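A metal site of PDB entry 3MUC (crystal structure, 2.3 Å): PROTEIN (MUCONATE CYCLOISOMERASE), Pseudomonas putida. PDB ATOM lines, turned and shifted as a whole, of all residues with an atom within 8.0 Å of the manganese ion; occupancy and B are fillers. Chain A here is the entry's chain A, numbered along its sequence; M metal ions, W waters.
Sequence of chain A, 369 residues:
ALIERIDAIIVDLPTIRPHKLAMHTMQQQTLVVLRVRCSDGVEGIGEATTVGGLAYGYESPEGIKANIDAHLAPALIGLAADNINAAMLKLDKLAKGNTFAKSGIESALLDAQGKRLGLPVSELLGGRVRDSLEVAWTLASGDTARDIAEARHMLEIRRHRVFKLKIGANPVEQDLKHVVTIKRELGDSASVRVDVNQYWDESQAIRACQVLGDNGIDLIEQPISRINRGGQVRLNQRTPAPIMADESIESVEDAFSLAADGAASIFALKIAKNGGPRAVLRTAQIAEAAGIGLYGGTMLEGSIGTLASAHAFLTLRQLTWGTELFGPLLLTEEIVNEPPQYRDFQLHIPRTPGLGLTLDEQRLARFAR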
ATOM      1  N   TYR A  56      18.330  18.286 -12.123  1.00  0.00           N
ATOM      2  CA  TYR A  56      17.714  17.596 -10.991  1.00  0.00           C
ATOM      3  C   TYR A  56      16.470  16.804 -11.391  1.00  0.00           C
ATOM      4  O   TYR A  56      15.687  16.376 -10.531  1.00  0.00           O
ATOM      5  CB  TYR A  56      17.390  18.583  -9.852  1.00  0.00           C
ATOM      6  CG  TYR A  56      18.611  19.147  -9.129  1.00  0.00           C
ATOM      7  CD1 TYR A  56      19.310  20.245  -9.640  1.00  0.00           C
ATOM      8  CD2 TYR A  56      19.067  18.575  -7.931  1.00  0.00           C
ATOM      9  CE1 TYR A  56      20.448  20.770  -8.972  1.00  0.00           C
ATOM     10  CE2 TYR A  56      20.204  19.093  -7.255  1.00  0.00           C
ATOM     11  CZ  TYR A  56      20.893  20.179  -7.780  1.00  0.00           C
ATOM     12  OH  TYR A  56      22.000  20.672  -7.121  1.00  0.00           O
ATOM     13  N   LYS A 164      19.027  22.437   7.190  1.00  0.00           N
ATOM     14  CA  LYS A 164      19.489  21.484   6.224  1.00  0.00           C
ATOM     15  C   LYS A 164      20.746  21.972   5.519  1.00  0.00           C
ATOM     16  O   LYS A 164      20.832  23.131   5.110  1.00  0.00           O
ATOM     17  CB  LYS A 164      18.370  21.227   5.229  1.00  0.00           C
ATOM     18  CG  LYS A 164      18.590  20.081   4.294  1.00  0.00           C
ATOM     19  CD  LYS A 164      17.383  19.922   3.417  1.00  0.00           C
ATOM     20  CE  LYS A 164      17.778  19.476   2.042  1.00  0.00           C
ATOM     21  NZ  LYS A 164      16.623  18.878   1.328  1.00  0.00           N
ATOM     22  N   LYS A 166      23.462  21.259   2.380  1.00  0.00           N
ATOM     23  CA  LYS A 166      23.715  20.595   1.103  1.00  0.00           C
ATOM     24  C   LYS A 166      25.210  20.340   1.008  1.00  0.00           C
ATOM     25  O   LYS A 166      25.996  21.281   0.981  1.00  0.00           O
ATOM     26  CB  LYS A 166      23.319  21.480  -0.047  1.00  0.00           C
ATOM     27  CG  LYS A 166      21.862  21.731  -0.131  1.00  0.00           C
ATOM     28  CD  LYS A 166      21.461  21.402  -1.527  1.00  0.00           C
ATOM     29  CE  LYS A 166      19.997  21.634  -1.756  1.00  0.00           C
ATOM     30  NZ  LYS A 166      19.755  21.365  -3.189  1.00  0.00           N
ATOM     31  N   VAL A 194      21.496  16.679   6.718  1.00  0.00           N
ATOM     32  CA  VAL A 194      22.265  16.884   5.499  1.00  0.00           C
ATOM     33  C   VAL A 194      21.556  16.284   4.327  1.00  0.00           C
ATOM     34  O   VAL A 194      20.726  15.380   4.493  1.00  0.00           O
ATOM     35  CB  VAL A 194      23.697  16.254   5.535  1.00  0.00           C
ATOM     36  CG1 VAL A 194      24.540  16.953   6.550  1.00  0.00           C
ATOM     37  CG2 VAL A 194      23.655  14.765   5.803  1.00  0.00           C
ATOM     38  N   ASP A 195      21.963  16.730   3.154  1.00  0.00           N
ATOM     39  CA  ASP A 195      21.444  16.276   1.895  1.00  0.00           C
ATOM     40  C   ASP A 195      22.650  16.225   0.982  1.00  0.00           C
ATOM     41  O   ASP A 195      23.249  17.257   0.681  1.00  0.00           O
ATOM     42  CB  ASP A 195      20.410  17.253   1.376  1.00  0.00           C
ATOM     43  CG  ASP A 195      19.651  16.733   0.172  1.00  0.00           C
ATOM     44  OD1 ASP A 195      20.067  15.754  -0.477  1.00  0.00           O
ATOM     45  OD2 ASP A 195      18.611  17.326  -0.128  1.00  0.00           O
ATOM     46  N   VAL A 196      22.983  15.013   0.540  1.00  0.00           N
ATOM     47  CA  VAL A 196      24.138  14.791  -0.322  1.00  0.00           C
ATOM     48  C   VAL A 196      23.823  14.762  -1.833  1.00  0.00           C
ATOM     49  O   VAL A 196      24.731  14.628  -2.661  1.00  0.00           O
ATOM     50  CB  VAL A 196      24.906  13.524   0.087  1.00  0.00           C
ATOM     51  CG1 VAL A 196      26.347  13.595  -0.407  1.00  0.00           C
ATOM     52  CG2 VAL A 196      24.873  13.349   1.611  1.00  0.00           C
ATOM     53  N   ASN A 197      22.548  14.814  -2.169  1.00  0.00           N
ATOM     54  CA  ASN A 197      22.087  14.857  -3.556  1.00  0.00           C
ATOM     55  C   ASN A 197      22.753  13.849  -4.491  1.00  0.00           C
ATOM     56  O   ASN A 197      23.141  14.196  -5.593  1.00  0.00           O
ATOM     57  CB  ASN A 197      22.230  16.282  -4.119  1.00  0.00           C
ATOM     58  CG  ASN A 197      21.229  17.262  -3.518  1.00  0.00           C
ATOM     59  OD1 ASN A 197      20.070  17.322  -3.949  1.00  0.00           O
ATOM     60  ND2 ASN A 197      21.637  17.984  -2.471  1.00  0.00           N
ATOM     61  N   GLN A 198      22.859  12.602  -4.029  1.00  0.00           N
ATOM     62  CA  GLN A 198      23.455  11.517  -4.827  1.00  0.00           C
ATOM     63  C   GLN A 198      24.954  11.672  -5.117  1.00  0.00           C
ATOM     64  O   GLN A 198      25.511  10.879  -5.852  1.00  0.00           O
ATOM     65  CB  GLN A 198      22.714  11.338  -6.176  1.00  0.00           C
ATOM     66  CG  GLN A 198      21.209  11.028  -6.067  1.00  0.00           C
ATOM     67  CD  GLN A 198      20.590  10.614  -7.378  1.00  0.00           C
ATOM     68  OE1 GLN A 198      20.275   9.439  -7.593  1.00  0.00           O
ATOM     69  NE2 GLN A 198      20.375  11.580  -8.261  1.00  0.00           N
ATOM     70  N   GLU A 221      20.051  12.597   4.001  1.00  0.00           N
ATOM     71  CA  GLU A 221      19.214  12.515   2.825  1.00  0.00           C
ATOM     72  C   GLU A 221      19.974  12.133   1.545  1.00  0.00           C
ATOM     73  O   GLU A 221      20.972  12.770   1.196  1.00  0.00           O
ATOM     74  CB  GLU A 221      18.498  13.838   2.649  1.00  0.00           C
ATOM     75  CG  GLU A 221      17.529  13.919   1.490  1.00  0.00           C
ATOM     76  CD  GLU A 221      16.743  15.223   1.506  1.00  0.00           C
ATOM     77  OE1 GLU A 221      17.010  16.117   2.325  1.00  0.00           O
ATOM     78  OE2 GLU A 221      15.812  15.348   0.707  1.00  0.00           O
ATOM     79  N   GLN A 222      19.456  11.127   0.861  1.00  0.00           N
ATOM     80  CA  GLN A 222      20.014  10.611  -0.393  1.00  0.00           C
ATOM     81  C   GLN A 222      21.535  10.674  -0.527  1.00  0.00           C
ATOM     82  O   GLN A 222      22.056  11.328  -1.448  1.00  0.00           O
ATOM     83  CB  GLN A 222      19.373  11.317  -1.584  1.00  0.00           C
ATOM     84  CG  GLN A 222      19.607  10.598  -2.904  1.00  0.00           C
ATOM     85  CD  GLN A 222      18.638   9.468  -3.124  1.00  0.00           C
ATOM     86  OE1 GLN A 222      17.499   9.528  -2.668  1.00  0.00           O
ATOM     87  NE2 GLN A 222      19.081   8.434  -3.821  1.00  0.00           N
ATOM     88  N   MET A 244      17.179   8.878   4.308  1.00  0.00           N
ATOM     89  CA  MET A 244      15.971   9.350   3.660  1.00  0.00           C
ATOM     90  C   MET A 244      16.137   9.259   2.146  1.00  0.00           C
ATOM     91  O   MET A 244      17.175   9.629   1.619  1.00  0.00           O
ATOM     92  CB  MET A 244      15.667  10.776   4.061  1.00  0.00           C
ATOM     93  CG  MET A 244      14.650  11.457   3.176  1.00  0.00           C
ATOM     94  SD  MET A 244      13.770  12.765   3.964  1.00  0.00           S
ATOM     95  CE  MET A 244      14.875  14.029   3.933  1.00  0.00           C
ATOM     96  N   ALA A 245      15.117   8.738   1.477  1.00  0.00           N
ATOM     97  CA  ALA A 245      15.168   8.637   0.028  1.00  0.00           C
ATOM     98  C   ALA A 245      14.453   9.835  -0.591  1.00  0.00           C
ATOM     99  O   ALA A 245      13.412  10.276  -0.083  1.00  0.00           O
ATOM    100  CB  ALA A 245      14.526   7.338  -0.444  1.00  0.00           C
ATOM    101  N   ASP A 246      15.046  10.391  -1.648  1.00  0.00           N
ATOM    102  CA  ASP A 246      14.453  11.507  -2.377  1.00  0.00           C
ATOM    103  C   ASP A 246      14.508  11.219  -3.879  1.00  0.00           C
ATOM    104  O   ASP A 246      13.489  10.899  -4.466  1.00  0.00           O
ATOM    105  CB  ASP A 246      15.147  12.843  -2.070  1.00  0.00           C
ATOM    106  CG  ASP A 246      14.534  14.015  -2.848  1.00  0.00           C
ATOM    107  OD1 ASP A 246      13.599  13.825  -3.658  1.00  0.00           O
ATOM    108  OD2 ASP A 246      15.011  15.138  -2.664  1.00  0.00           O
ATOM    109  N   GLU A 247      15.694  11.328  -4.473  1.00  0.00           N
ATOM    110  CA  GLU A 247      15.853  11.070  -5.912  1.00  0.00           C
ATOM    111  C   GLU A 247      15.515   9.651  -6.324  1.00  0.00           C
ATOM    112  O   GLU A 247      15.214   9.401  -7.483  1.00  0.00           O
ATOM    113  CB  GLU A 247      17.261  11.412  -6.404  1.00  0.00           C
ATOM    114  CG  GLU A 247      17.505  12.895  -6.650  1.00  0.00           C
ATOM    115  CD  GLU A 247      17.715  13.689  -5.378  1.00  0.00           C
ATOM    116  OE1 GLU A 247      18.074  13.094  -4.348  1.00  0.00           O
ATOM    117  OE2 GLU A 247      17.518  14.905  -5.425  1.00  0.00           O
ATOM    118  N   ALA A 268      11.021  11.183   1.188  1.00  0.00           N
ATOM    119  CA  ALA A 268      10.740  12.594   0.989  1.00  0.00           C
ATOM    120  C   ALA A 268       9.540  12.579   0.042  1.00  0.00           C
ATOM    121  O   ALA A 268       9.501  11.793  -0.907  1.00  0.00           O
ATOM    122  CB  ALA A 268      11.921  13.306   0.344  1.00  0.00           C
ATOM    123  N   LYS A 270       7.418  14.569  -2.685  1.00  0.00           N
ATOM    124  CA  LYS A 270       7.402  15.718  -3.573  1.00  0.00           C
ATOM    125  C   LYS A 270       6.304  15.529  -4.612  1.00  0.00           C
ATOM    126  O   LYS A 270       6.304  14.542  -5.353  1.00  0.00           O
ATOM    127  CB  LYS A 270       8.746  15.901  -4.275  1.00  0.00           C
ATOM    128  CG  LYS A 270       9.890  16.189  -3.327  1.00  0.00           C
ATOM    129  CD  LYS A 270      11.161  16.439  -4.077  1.00  0.00           C
ATOM    130  CE  LYS A 270      12.266  16.827  -3.126  1.00  0.00           C
ATOM    131  NZ  LYS A 270      13.516  17.239  -3.836  1.00  0.00           N
ATOM    132  N   TYR A 295       8.437  13.039   5.274  1.00  0.00           N
ATOM    133  CA  TYR A 295       9.031  14.363   5.226  1.00  0.00           C
ATOM    134  C   TYR A 295       8.468  15.060   3.999  1.00  0.00           C
ATOM    135  O   TYR A 295       8.479  14.496   2.910  1.00  0.00           O
ATOM    136  CB  TYR A 295      10.549  14.221   5.090  1.00  0.00           C
ATOM    137  CG  TYR A 295      11.309  15.519   4.938  1.00  0.00           C
ATOM    138  CD1 TYR A 295      11.445  16.404   6.002  1.00  0.00           C
ATOM    139  CD2 TYR A 295      11.951  15.828   3.738  1.00  0.00           C
ATOM    140  CE1 TYR A 295      12.245  17.556   5.886  1.00  0.00           C
ATOM    141  CE2 TYR A 295      12.746  16.975   3.616  1.00  0.00           C
ATOM    142  CZ  TYR A 295      12.882  17.829   4.692  1.00  0.00           C
ATOM    143  OH  TYR A 295      13.720  18.914   4.590  1.00  0.00           O
ATOM    144  N   GLY A 297       8.819  17.336   1.127  1.00  0.00           N
ATOM    145  CA  GLY A 297       9.851  17.942   0.321  1.00  0.00           C
ATOM    146  C   GLY A 297       9.361  18.961  -0.678  1.00  0.00           C
ATOM    147  O   GLY A 297       8.144  19.133  -0.873  1.00  0.00           O
ATOM    148  N   THR A 298      10.308  19.600  -1.357  1.00  0.00           N
ATOM    149  CA  THR A 298      10.000  20.640  -2.326  1.00  0.00           C
ATOM    150  C   THR A 298      11.037  20.649  -3.440  1.00  0.00           C
ATOM    151  O   THR A 298      12.120  20.091  -3.294  1.00  0.00           O
ATOM    152  CB  THR A 298      10.018  22.044  -1.629  1.00  0.00           C
ATOM    153  OG1 THR A 298       9.556  23.045  -2.540  1.00  0.00           O
ATOM    154  CG2 THR A 298      11.445  22.436  -1.169  1.00  0.00           C
ATOM    155  N   MET A 299      10.647  21.239  -4.565  1.00  0.00           N
ATOM    156  CA  MET A 299      11.546  21.429  -5.715  1.00  0.00           C
ATOM    157  C   MET A 299      11.780  22.946  -5.861  1.00  0.00           C
ATOM    158  O   MET A 299      12.018  23.449  -6.957  1.00  0.00           O
ATOM    159  CB  MET A 299      10.925  20.859  -6.996  1.00  0.00           C
ATOM    160  CG  MET A 299      10.838  19.330  -7.042  1.00  0.00           C
ATOM    161  SD  MET A 299      12.429  18.425  -6.930  1.00  0.00           S
ATOM    162  CE  MET A 299      13.316  19.018  -8.396  1.00  0.00           C
ATOM    163  N   GLU A 324      10.045  21.056   4.249  1.00  0.00           N
ATOM    164  CA  GLU A 324      11.003  22.066   3.818  1.00  0.00           C
ATOM    165  C   GLU A 324      10.324  22.998   2.810  1.00  0.00           C
ATOM    166  O   GLU A 324      10.941  23.418   1.838  1.00  0.00           O
ATOM    167  CB  GLU A 324      12.248  21.422   3.213  1.00  0.00           C
ATOM    168  CG  GLU A 324      11.948  20.543   2.023  1.00  0.00           C
ATOM    169  CD  GLU A 324      13.174  19.880   1.464  1.00  0.00           C
ATOM    170  OE1 GLU A 324      14.214  19.868   2.157  1.00  0.00           O
ATOM    171  OE2 GLU A 324      13.099  19.358   0.327  1.00  0.00           O
HETATM  172 MN    MN M   1      16.873  16.097  -1.500  1.00  0.00          MN
HETATM  173  O   HOH W   1      15.540  18.031  -1.409  1.00  0.00           O
HETATM  174  O   HOH W   2      18.274  14.302  -2.117  1.00  0.00           O
HETATM  175  O   HOH W   3      17.078  17.299  -3.459  1.00  0.00           O
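The side-chain carboxylate (OD1) of Asp 246 is in salt-bridge range of the side-chain amino group (NZ) of Lys 270.
N of Asp 246 is in hydrogen-bond range of OE1 of Gln 222, 2.8 Å away.
The side-chain carboxylate (OD2) of Asp 195 lies close to the side-chain amino group (NZ) of Lys 164, at 2.9 Å.
The backbone NH (N) of Asn 197 lies within hydrogen-bond range of the side-chain carboxylate (OD1) of Asp 195 (3.1 Å).
The side-chain carboxylate of Glu 221 is in salt-bridge range of the side-chain amino group of Lys 164 (3.0 Å).
N of Val 196 lies within hydrogen-bond range of O of Glu 221 (3.1 Å).
N of Glu 221 lies within hydrogen-bond range of O of Val 194, 2.9 Å away.
The side-chain amino group (NZ) of Lys 164 lies within salt-bridge range of the side-chain carboxylate (OE1) of Glu 324.
Lys 164 touches the manganese ion (NZ to MN, 3.97 Å).
Of the 21 residues printed, 4 come within 4 Å of the manganese ion.
The nearest printed residue that does not touch the manganese ion is Glu 247 (4.2 Å).
The manganese ion is bound by water W3 (2.3 Å), water W1 (2.4 Å), water W2 (2.4 Å), OD2 of Asp 246 (2.4 Å), OD2 of Asp 195 (2.5 Å) and OE2 of Glu 221 (2.6 Å).
Water W2 lies within hydrogen-bond range of the side-chain carboxylate (OE1) of Glu 247 (2.5 Å) and the side-chain carboxylate (OD1) of Asp 195 (2.8 Å).
Water W1 lies within hydrogen-bond range of the side-chain amino group of Lys 164 (3.1 Å), the side-chain amino group of Lys 270 (3.3 Å) and the side-chain carboxylate of Glu 324 (3.3 Å).
Water W3 lies within hydrogen-bond range of the side-chain amide oxygen (OD1) of Asn 197 and the side-chain carboxylate (OE2) of Glu 247.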
